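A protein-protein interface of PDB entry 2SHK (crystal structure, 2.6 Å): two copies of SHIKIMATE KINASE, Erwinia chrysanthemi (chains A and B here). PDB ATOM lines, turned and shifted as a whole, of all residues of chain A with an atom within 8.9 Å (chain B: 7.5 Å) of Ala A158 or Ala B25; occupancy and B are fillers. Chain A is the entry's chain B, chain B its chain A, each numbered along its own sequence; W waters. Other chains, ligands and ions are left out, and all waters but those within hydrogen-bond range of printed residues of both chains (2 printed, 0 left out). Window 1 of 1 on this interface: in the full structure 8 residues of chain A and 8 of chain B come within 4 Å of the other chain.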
ATOM      1  N   THR A  17      11.827  16.107   5.796  1.00  0.00           N
ATOM      2  CA  THR A  17      12.987  15.721   5.017  1.00  0.00           C
ATOM      3  C   THR A  17      12.635  14.925   3.782  1.00  0.00           C
ATOM      4  O   THR A  17      12.967  15.229   2.643  1.00  0.00           O
ATOM      5  CB  THR A  17      13.942  14.933   5.939  1.00  0.00           C
ATOM      6  OG1 THR A  17      14.807  15.905   6.597  1.00  0.00           O
ATOM      7  CG2 THR A  17      14.838  13.947   5.230  1.00  0.00           C
ATOM      8  N   VAL A  18      11.865  13.876   4.107  1.00  0.00           N
ATOM      9  CA  VAL A  18      11.323  13.001   3.068  1.00  0.00           C
ATOM     10  C   VAL A  18      10.273  13.770   2.275  1.00  0.00           C
ATOM     11  O   VAL A  18      10.255  13.560   1.067  1.00  0.00           O
ATOM     12  CB  VAL A  18      10.724  11.716   3.617  1.00  0.00           C
ATOM     13  CG1 VAL A  18      10.012  10.920   2.534  1.00  0.00           C
ATOM     14  CG2 VAL A  18      11.808  10.900   4.302  1.00  0.00           C
ATOM     15  N   GLU A  21      12.108  15.954  -0.258  1.00  0.00           N
ATOM     16  CA  GLU A  21      12.721  15.162  -1.314  1.00  0.00           C
ATOM     17  C   GLU A  21      11.651  14.665  -2.269  1.00  0.00           C
ATOM     18  O   GLU A  21      11.861  14.760  -3.475  1.00  0.00           O
ATOM     19  CB  GLU A  21      13.632  14.032  -0.868  1.00  0.00           C
ATOM     20  CG  GLU A  21      14.906  14.485  -0.184  1.00  0.00           C
ATOM     21  CD  GLU A  21      15.392  15.859  -0.629  1.00  0.00           C
ATOM     22  OE1 GLU A  21      15.696  16.041  -1.827  1.00  0.00           O
ATOM     23  OE2 GLU A  21      15.412  16.718   0.275  1.00  0.00           O
ATOM     24  N   LEU A  22      10.508  14.271  -1.746  1.00  0.00           N
ATOM     25  CA  LEU A  22       9.454  13.800  -2.635  1.00  0.00           C
ATOM     26  C   LEU A  22       8.920  14.905  -3.530  1.00  0.00           C
ATOM     27  O   LEU A  22       8.714  14.741  -4.719  1.00  0.00           O
ATOM     28  CB  LEU A  22       8.401  13.010  -1.831  1.00  0.00           C
ATOM     29  CG  LEU A  22       7.268  12.525  -2.738  1.00  0.00           C
ATOM     30  CD1 LEU A  22       7.715  11.456  -3.722  1.00  0.00           C
ATOM     31  CD2 LEU A  22       6.094  12.096  -1.875  1.00  0.00           C
ATOM     32  N   ARG A  24      10.450  17.650  -4.454  1.00  0.00           N
ATOM     33  CA  ARG A  24      11.553  17.925  -5.356  1.00  0.00           C
ATOM     34  C   ARG A  24      11.546  16.910  -6.486  1.00  0.00           C
ATOM     35  O   ARG A  24      11.489  17.278  -7.673  1.00  0.00           O
ATOM     36  CB  ARG A  24      12.898  17.969  -4.635  1.00  0.00           C
ATOM     37  CG  ARG A  24      14.055  18.113  -5.620  1.00  0.00           C
ATOM     38  CD  ARG A  24      15.112  19.072  -5.089  1.00  0.00           C
ATOM     39  NE  ARG A  24      16.105  19.410  -6.142  1.00  0.00           N
ATOM     40  CZ  ARG A  24      17.049  20.338  -5.903  1.00  0.00           C
ATOM     41  NH1 ARG A  24      17.072  20.943  -4.714  1.00  0.00           N
ATOM     42  NH2 ARG A  24      17.974  20.662  -6.806  1.00  0.00           N
ATOM     43  N   ALA A  25      11.484  15.631  -6.185  1.00  0.00           N
ATOM     44  CA  ALA A  25      11.444  14.628  -7.233  1.00  0.00           C
ATOM     45  C   ALA A  25      10.232  14.810  -8.112  1.00  0.00           C
ATOM     46  O   ALA A  25      10.336  14.411  -9.263  1.00  0.00           O
ATOM     47  CB  ALA A  25      11.454  13.211  -6.708  1.00  0.00           C
ATOM     48  N   GLN A 155      14.881   3.621   5.927  1.00  0.00           N
ATOM     49  CA  GLN A 155      15.684   3.815   4.742  1.00  0.00           C
ATOM     50  C   GLN A 155      16.027   5.306   4.632  1.00  0.00           C
ATOM     51  O   GLN A 155      15.350   6.119   5.225  1.00  0.00           O
ATOM     52  CB  GLN A 155      14.874   3.407   3.497  1.00  0.00           C
ATOM     53  CG  GLN A 155      14.420   1.984   3.357  1.00  0.00           C
ATOM     54  CD  GLN A 155      13.451   1.772   2.246  1.00  0.00           C
ATOM     55  OE1 GLN A 155      13.731   1.437   1.089  1.00  0.00           O
ATOM     56  NE2 GLN A 155      12.179   1.962   2.548  1.00  0.00           N
ATOM     57  N   PRO A 156      17.082   5.653   3.919  1.00  0.00           N
ATOM     58  CA  PRO A 156      17.467   7.009   3.601  1.00  0.00           C
ATOM     59  C   PRO A 156      16.379   7.662   2.743  1.00  0.00           C
ATOM     60  O   PRO A 156      15.697   6.950   2.003  1.00  0.00           O
ATOM     61  CB  PRO A 156      18.735   6.895   2.740  1.00  0.00           C
ATOM     62  CG  PRO A 156      19.151   5.490   2.860  1.00  0.00           C
ATOM     63  CD  PRO A 156      17.948   4.668   3.188  1.00  0.00           C
ATOM     64  N   PRO A 157      16.302   8.975   2.728  1.00  0.00           N
ATOM     65  CA  PRO A 157      15.217   9.667   2.105  1.00  0.00           C
ATOM     66  C   PRO A 157      15.036   9.401   0.639  1.00  0.00           C
ATOM     67  O   PRO A 157      13.912   9.224   0.138  1.00  0.00           O
ATOM     68  CB  PRO A 157      15.471  11.135   2.423  1.00  0.00           C
ATOM     69  CG  PRO A 157      16.296  11.143   3.645  1.00  0.00           C
ATOM     70  CD  PRO A 157      17.100   9.853   3.617  1.00  0.00           C
ATOM     71  N   ALA A 158      16.141   9.403  -0.086  1.00  0.00           N
ATOM     72  CA  ALA A 158      16.072   9.219  -1.538  1.00  0.00           C
ATOM     73  C   ALA A 158      15.596   7.813  -1.846  1.00  0.00           C
ATOM     74  O   ALA A 158      15.094   7.603  -2.947  1.00  0.00           O
ATOM     75  CB  ALA A 158      17.354   9.630  -2.238  1.00  0.00           C
ATOM     76  N   ALA A 159      15.806   6.829  -0.986  1.00  0.00           N
ATOM     77  CA  ALA A 159      15.264   5.492  -1.224  1.00  0.00           C
ATOM     78  C   ALA A 159      13.758   5.459  -0.912  1.00  0.00           C
ATOM     79  O   ALA A 159      13.020   4.758  -1.583  1.00  0.00           O
ATOM     80  CB  ALA A 159      15.871   4.393  -0.398  1.00  0.00           C
ATOM     81  N   ILE A 160      13.352   6.161   0.144  1.00  0.00           N
ATOM     82  CA  ILE A 160      11.949   6.234   0.484  1.00  0.00           C
ATOM     83  C   ILE A 160      11.244   6.846  -0.732  1.00  0.00           C
ATOM     84  O   ILE A 160      10.271   6.259  -1.190  1.00  0.00           O
ATOM     85  CB  ILE A 160      11.733   7.107   1.739  1.00  0.00           C
ATOM     86  CG1 ILE A 160      12.453   6.431   2.902  1.00  0.00           C
ATOM     87  CG2 ILE A 160      10.245   7.285   1.962  1.00  0.00           C
ATOM     88  CD1 ILE A 160      12.352   7.195   4.214  1.00  0.00           C
ATOM     89  N   VAL A 161      11.747   7.960  -1.245  1.00  0.00           N
ATOM     90  CA  VAL A 161      11.169   8.549  -2.443  1.00  0.00           C
ATOM     91  C   VAL A 161      11.050   7.581  -3.613  1.00  0.00           C
ATOM     92  O   VAL A 161       9.941   7.541  -4.182  1.00  0.00           O
ATOM     93  CB  VAL A 161      11.979   9.749  -2.939  1.00  0.00           C
ATOM     94  CG1 VAL A 161      11.498  10.334  -4.217  1.00  0.00           C
ATOM     95  CG2 VAL A 161      11.882  10.757  -1.817  1.00  0.00           C
ATOM     96  N   CYS A 162      12.112   6.879  -3.960  1.00  0.00           N
ATOM     97  CA  CYS A 162      12.078   5.869  -5.004  1.00  0.00           C
ATOM     98  C   CYS A 162      11.023   4.803  -4.756  1.00  0.00           C
ATOM     99  O   CYS A 162      10.288   4.470  -5.697  1.00  0.00           O
ATOM    100  CB  CYS A 162      13.473   5.187  -5.207  1.00  0.00           C
ATOM    101  SG  CYS A 162      14.644   6.317  -5.999  1.00  0.00           S
ATOM    102  N   GLU A 163      10.905   4.313  -3.533  1.00  0.00           N
ATOM    103  CA  GLU A 163       9.912   3.291  -3.206  1.00  0.00           C
ATOM    104  C   GLU A 163       8.513   3.868  -3.397  1.00  0.00           C
ATOM    105  O   GLU A 163       7.639   3.170  -3.936  1.00  0.00           O
ATOM    106  CB  GLU A 163      10.020   2.693  -1.791  1.00  0.00           C
ATOM    107  CG  GLU A 163       9.026   1.625  -1.448  1.00  0.00           C
ATOM    108  CD  GLU A 163       9.224   0.931  -0.082  1.00  0.00           C
ATOM    109  OE1 GLU A 163      10.438   0.921   0.388  1.00  0.00           O
ATOM    110  OE2 GLU A 163       8.152   0.456   0.455  1.00  0.00           O
ATOM    111  N   LEU A 164       8.364   5.105  -2.886  1.00  0.00           N
ATOM    112  CA  LEU A 164       7.040   5.717  -2.941  1.00  0.00           C
ATOM    113  C   LEU A 164       6.649   5.987  -4.366  1.00  0.00           C
ATOM    114  O   LEU A 164       5.526   5.697  -4.739  1.00  0.00           O
ATOM    115  CB  LEU A 164       6.919   6.987  -2.094  1.00  0.00           C
ATOM    116  CG  LEU A 164       7.018   6.789  -0.592  1.00  0.00           C
ATOM    117  CD1 LEU A 164       7.056   8.132   0.100  1.00  0.00           C
ATOM    118  CD2 LEU A 164       5.829   6.001  -0.101  1.00  0.00           C
ATOM    119  N   MET A 165       7.579   6.406  -5.219  1.00  0.00           N
ATOM    120  CA  MET A 165       7.248   6.615  -6.634  1.00  0.00           C
ATOM    121  C   MET A 165       6.828   5.334  -7.322  1.00  0.00           C
ATOM    122  O   MET A 165       5.832   5.398  -8.047  1.00  0.00           O
ATOM    123  CB  MET A 165       8.383   7.273  -7.400  1.00  0.00           C
ATOM    124  CG  MET A 165       8.372   8.755  -7.001  1.00  0.00           C
ATOM    125  SD  MET A 165       9.507   9.639  -8.056  1.00  0.00           S
ATOM    126  CE  MET A 165      10.973   8.674  -7.578  1.00  0.00           C
ATOM    127  N   GLY B  19      22.375  14.534 -13.587  1.00  0.00           N
ATOM    128  CA  GLY B  19      23.599  14.599 -12.839  1.00  0.00           C
ATOM    129  C   GLY B  19      23.398  15.304 -11.487  1.00  0.00           C
ATOM    130  O   GLY B  19      23.904  14.831 -10.458  1.00  0.00           O
ATOM    131  N   ARG B  20      22.729  16.464 -11.526  1.00  0.00           N
ATOM    132  CA  ARG B  20      22.528  17.206 -10.282  1.00  0.00           C
ATOM    133  C   ARG B  20      21.549  16.465  -9.383  1.00  0.00           C
ATOM    134  O   ARG B  20      21.771  16.340  -8.174  1.00  0.00           O
ATOM    135  CB  ARG B  20      22.136  18.642 -10.575  1.00  0.00           C
ATOM    136  CG  ARG B  20      21.530  19.393  -9.395  1.00  0.00           C
ATOM    137  CD  ARG B  20      20.715  20.605  -9.865  1.00  0.00           C
ATOM    138  NE  ARG B  20      21.652  21.545 -10.470  1.00  0.00           N
ATOM    139  CZ  ARG B  20      21.678  21.941 -11.765  1.00  0.00           C
ATOM    140  NH1 ARG B  20      20.707  21.439 -12.541  1.00  0.00           N
ATOM    141  NH2 ARG B  20      22.680  22.809 -12.101  1.00  0.00           N
ATOM    142  N   GLU B  21      20.524  15.854  -9.972  1.00  0.00           N
ATOM    143  CA  GLU B  21      19.544  15.112  -9.187  1.00  0.00           C
ATOM    144  C   GLU B  21      20.148  13.854  -8.579  1.00  0.00           C
ATOM    145  O   GLU B  21      19.819  13.473  -7.462  1.00  0.00           O
ATOM    146  CB  GLU B  21      18.254  14.905  -9.999  1.00  0.00           C
ATOM    147  CG  GLU B  21      17.433  16.150 -10.302  1.00  0.00           C
ATOM    148  CD  GLU B  21      17.370  17.107  -9.146  1.00  0.00           C
ATOM    149  OE1 GLU B  21      17.083  16.696  -8.024  1.00  0.00           O
ATOM    150  OE2 GLU B  21      17.676  18.295  -9.272  1.00  0.00           O
ATOM    151  N   LEU B  22      21.112  13.203  -9.247  1.00  0.00           N
ATOM    152  CA  LEU B  22      21.715  11.986  -8.705  1.00  0.00           C
ATOM    153  C   LEU B  22      22.651  12.277  -7.566  1.00  0.00           C
ATOM    154  O   LEU B  22      22.785  11.637  -6.538  1.00  0.00           O
ATOM    155  CB  LEU B  22      22.447  11.298  -9.853  1.00  0.00           C
ATOM    156  CG  LEU B  22      23.332  10.099  -9.540  1.00  0.00           C
ATOM    157  CD1 LEU B  22      22.456   8.917  -9.166  1.00  0.00           C
ATOM    158  CD2 LEU B  22      24.216   9.726 -10.730  1.00  0.00           C
ATOM    159  N   ALA B  23      23.357  13.403  -7.674  1.00  0.00           N
ATOM    160  CA  ALA B  23      24.309  13.880  -6.690  1.00  0.00           C
ATOM    161  C   ALA B  23      23.548  14.118  -5.376  1.00  0.00           C
ATOM    162  O   ALA B  23      24.089  13.869  -4.318  1.00  0.00           O
ATOM    163  CB  ALA B  23      24.998  15.163  -7.085  1.00  0.00           C
ATOM    164  N   ARG B  24      22.343  14.671  -5.516  1.00  0.00           N
ATOM    165  CA  ARG B  24      21.584  15.006  -4.315  1.00  0.00           C
ATOM    166  C   ARG B  24      21.195  13.711  -3.623  1.00  0.00           C
ATOM    167  O   ARG B  24      21.406  13.557  -2.427  1.00  0.00           O
ATOM    168  CB  ARG B  24      20.389  15.893  -4.587  1.00  0.00           C
ATOM    169  CG  ARG B  24      19.540  16.176  -3.367  1.00  0.00           C
ATOM    170  CD  ARG B  24      18.146  16.614  -3.756  1.00  0.00           C
ATOM    171  NE  ARG B  24      17.593  17.652  -2.938  1.00  0.00           N
ATOM    172  CZ  ARG B  24      18.001  18.876  -2.675  1.00  0.00           C
ATOM    173  NH1 ARG B  24      19.110  19.390  -3.176  1.00  0.00           N
ATOM    174  NH2 ARG B  24      17.245  19.622  -1.874  1.00  0.00           N
ATOM    175  N   ALA B  25      20.759  12.736  -4.381  1.00  0.00           N
ATOM    176  CA  ALA B  25      20.282  11.508  -3.809  1.00  0.00           C
ATOM    177  C   ALA B  25      21.355  10.735  -3.086  1.00  0.00           C
ATOM    178  O   ALA B  25      21.053   9.973  -2.177  1.00  0.00           O
ATOM    179  CB  ALA B  25      19.584  10.694  -4.902  1.00  0.00           C
ATOM    180  N   LEU B  26      22.556  10.817  -3.537  1.00  0.00           N
ATOM    181  CA  LEU B  26      23.701  10.112  -3.034  1.00  0.00           C
ATOM    182  C   LEU B  26      24.491  10.910  -2.001  1.00  0.00           C
ATOM    183  O   LEU B  26      25.332  10.381  -1.291  1.00  0.00           O
ATOM    184  CB  LEU B  26      24.694   9.837  -4.198  1.00  0.00           C
ATOM    185  CG  LEU B  26      24.186   9.041  -5.392  1.00  0.00           C
ATOM    186  CD1 LEU B  26      25.234   9.026  -6.499  1.00  0.00           C
ATOM    187  CD2 LEU B  26      23.863   7.611  -4.997  1.00  0.00           C
ATOM    188  N   GLY B  27      24.212  12.164  -1.909  1.00  0.00           N
ATOM    189  CA  GLY B  27      24.901  13.112  -1.059  1.00  0.00           C
ATOM    190  C   GLY B  27      26.244  13.480  -1.665  1.00  0.00           C
ATOM    191  O   GLY B  27      27.239  13.663  -1.010  1.00  0.00           O
ATOM    192  N   TYR B  28      26.340  13.546  -3.005  1.00  0.00           N
ATOM    193  CA  TYR B  28      27.630  13.852  -3.601  1.00  0.00           C
ATOM    194  C   TYR B  28      27.715  15.302  -3.962  1.00  0.00           C
ATOM    195  O   TYR B  28      26.734  16.028  -4.038  1.00  0.00           O
ATOM    196  CB  TYR B  28      27.711  12.986  -4.857  1.00  0.00           C
ATOM    197  CG  TYR B  28      28.167  11.562  -4.706  1.00  0.00           C
ATOM    198  CD1 TYR B  28      28.188  10.899  -3.494  1.00  0.00           C
ATOM    199  CD2 TYR B  28      28.601  10.887  -5.812  1.00  0.00           C
ATOM    200  CE1 TYR B  28      28.586   9.607  -3.397  1.00  0.00           C
ATOM    201  CE2 TYR B  28      29.050   9.579  -5.723  1.00  0.00           C
ATOM    202  CZ  TYR B  28      29.018   8.939  -4.504  1.00  0.00           C
ATOM    203  OH  TYR B  28      29.471   7.629  -4.455  1.00  0.00           O
ATOM    204  N   ALA B 158      13.911  11.926 -12.041  1.00  0.00           N
ATOM    205  CA  ALA B 158      13.803  11.188 -10.807  1.00  0.00           C
ATOM    206  C   ALA B 158      13.839   9.689 -11.008  1.00  0.00           C
ATOM    207  O   ALA B 158      14.330   8.921 -10.185  1.00  0.00           O
ATOM    208  CB  ALA B 158      12.462  11.491 -10.120  1.00  0.00           C
ATOM    209  N   VAL B 161      17.366   8.589 -11.765  1.00  0.00           N
ATOM    210  CA  VAL B 161      18.120   8.567 -10.525  1.00  0.00           C
ATOM    211  C   VAL B 161      17.873   7.273  -9.776  1.00  0.00           C
ATOM    212  O   VAL B 161      18.811   6.573  -9.347  1.00  0.00           O
ATOM    213  CB  VAL B 161      17.855   9.788  -9.669  1.00  0.00           C
ATOM    214  CG1 VAL B 161      18.452   9.708  -8.259  1.00  0.00           C
ATOM    215  CG2 VAL B 161      18.330  11.090 -10.309  1.00  0.00           C
ATOM    216  N   CYS B 162      16.621   6.887  -9.718  1.00  0.00           N
ATOM    217  CA  CYS B 162      16.173   5.651  -9.068  1.00  0.00           C
ATOM    218  C   CYS B 162      16.732   4.445  -9.773  1.00  0.00           C
ATOM    219  O   CYS B 162      17.349   3.556  -9.180  1.00  0.00           O
ATOM    220  CB  CYS B 162      14.630   5.698  -9.047  1.00  0.00           C
ATOM    221  SG  CYS B 162      13.972   6.889  -7.809  1.00  0.00           S
ATOM    222  N   MET B 165      20.449   4.277  -9.073  1.00  0.00           N
ATOM    223  CA  MET B 165      20.858   3.708  -7.758  1.00  0.00           C
ATOM    224  C   MET B 165      20.733   2.193  -7.692  1.00  0.00           C
ATOM    225  O   MET B 165      21.583   1.468  -7.165  1.00  0.00           O
ATOM    226  CB  MET B 165      20.136   4.432  -6.623  1.00  0.00           C
ATOM    227  CG  MET B 165      20.547   5.928  -6.610  1.00  0.00           C
ATOM    228  SD  MET B 165      19.926   6.662  -5.061  1.00  0.00           S
ATOM    229  CE  MET B 165      18.187   6.443  -5.478  1.00  0.00           C
ATOM    230  N   LEU B 170      24.151   1.828  -5.578  1.00  0.00           N
ATOM    231  CA  LEU B 170      24.548   2.977  -4.796  1.00  0.00           C
ATOM    232  C   LEU B 170      23.480   3.223  -3.725  1.00  0.00           C
ATOM    233  O   LEU B 170      22.278   3.250  -3.978  1.00  0.00           O
ATOM    234  CB  LEU B 170      24.760   4.222  -5.625  1.00  0.00           C
ATOM    235  CG  LEU B 170      25.966   4.053  -6.556  1.00  0.00           C
ATOM    236  CD1 LEU B 170      25.813   5.023  -7.758  1.00  0.00           C
ATOM    237  CD2 LEU B 170      27.283   4.228  -5.801  1.00  0.00           C
ATOM    238  N   PRO B 171      23.986   3.374  -2.511  1.00  0.00           N
ATOM    239  CA  PRO B 171      23.159   3.718  -1.349  1.00  0.00           C
ATOM    240  C   PRO B 171      22.796   5.192  -1.406  1.00  0.00           C
ATOM    241  O   PRO B 171      23.611   5.949  -1.952  1.00  0.00           O
ATOM    242  CB  PRO B 171      24.108   3.448  -0.173  1.00  0.00           C
ATOM    243  CG  PRO B 171      25.479   3.713  -0.673  1.00  0.00           C
ATOM    244  CD  PRO B 171      25.440   3.455  -2.162  1.00  0.00           C
ATOM    245  N   ALA B 172      21.699   5.559  -0.776  1.00  0.00           N
ATOM    246  CA  ALA B 172      21.358   6.991  -0.729  1.00  0.00           C
ATOM    247  C   ALA B 172      21.964   7.685   0.491  1.00  0.00           C
ATOM    248  O   ALA B 172      22.344   7.056   1.483  1.00  0.00           O
ATOM    249  CB  ALA B 172      19.846   7.051  -0.893  1.00  0.00           C
ATOM    250  N   ALA B 173      22.162   8.992   0.431  1.00  0.00           N
ATOM    251  CA  ALA B 173      22.683   9.850   1.475  1.00  0.00           C
ATOM    252  C   ALA B 173      21.992   9.601   2.835  1.00  0.00           C
ATOM    253  O   ALA B 173      22.749   9.228   3.798  1.00  0.00           O
ATOM    254  CB  ALA B 173      22.520  11.317   1.073  1.00  0.00           C
ATOM    255  OXT ALA B 173      20.739   9.742   2.954  1.00  0.00           O
HETATM  256  O   HOH W   1      19.175  10.020   0.663  1.00  0.00           O
HETATM  257  O   HOH W   2      20.739  20.179  -5.183  1.00  0.00           O
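SG of Cys B162 is disulfide-bonded to SG of Cys A162 (2.0 Å).
The guanidinium group of Arg A24 sits close to the guanidinium group of Arg B24 (3.0 Å).
NE of Arg B24 is in salt-bridge range of OE1 of Glu A21 (2.7 Å).
The side-chain carboxylate (OE2) of Glu B21 lies within salt-bridge range of the guanidinium group (NH2) of Arg A24 (3.4 Å).
The backbone carbonyl oxygen of Ala B25 lies within hydrogen-bond range of the backbone NH of Ala B173.
The backbone NH of Leu B170 lies within hydrogen-bond range of the backbone carbonyl oxygen of Met B165 (3.0 Å).
Among the printed residues, merely in contact across the chains: Ala A25 with Ala B158 (3.7 Å), Pro A156 with Ala B172 (3.8 Å), Pro A156 with Ala B173 (3.5 Å), Pro A157 with Ala B173 (3.7 Å), Ala A158 with Ala B25 (3.6 Å), Ala A158 with Ala B172 (3.8 Å), Cys A162 with Met B165 (3.6 Å) and Met A165 with Cys B162 (3.5 Å).
Ala A158 touches just these residues of chain B: Ala B25 and Ala B172.
Ala B25 touches one residue of chain A.
Of the printed residues of chain B, Pro A157 touches Ala B173.
Of the printed residues of chain B, Cys A162 touches Cys B162 (2.0 Å) and Met B165 (3.6 Å).
Of the printed residues of chain B, Pro A156 touches Ala B172 (3.8 Å) and Ala B173 (3.5 Å).
Printed residues of chain A within 4 Å of Ala B172: Pro A156 (3.8 Å) and Ala A158 (3.8 Å).
Printed residues of chain B within 4 Å of Glu A21: Arg B24.
The nearest residue of chain B that does not touch Ala A158 is Met B165 (4.2 Å).
Printed residues of chain B that touch a printed residue of chain A: Glu B21, Arg B24, Ala B25, Ala B158, Cys B162, Met B165, Ala B172 and Ala B173.
Hydrophobic or aromatic side chains of chain B within 4 Å of the printed part of chain A: Ala B25, Ala B158, Met B165 and Ala B172.
Glu A21 touches Arg B24, and with the chains exchanged Arg A24 touches Glu B21.
Arg A24 touches its own counterpart, Arg B24.
Ala A25 touches Ala B158, and with the chains exchanged Ala A158 touches Ala B25.
Cys A162 touches Met B165, and with the chains exchanged Met A165 touches Cys B162.
Of the 12 pairs that touch across the chains among the printed residues, 8 have their exchanged pair printed and touching as well.
Water W2 lies within hydrogen-bond range of the guanidinium group of Arg B24 (2.7 Å) and the guanidinium group of Arg A24 (3.2 Å).
Water W1 lies within hydrogen-bond range of the chain-end carboxylate of Ala B173 (2.8 Å), the backbone NH of Ala A158 (3.2 Å) and the backbone carbonyl oxygen of Ala B25 (3.4 Å).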
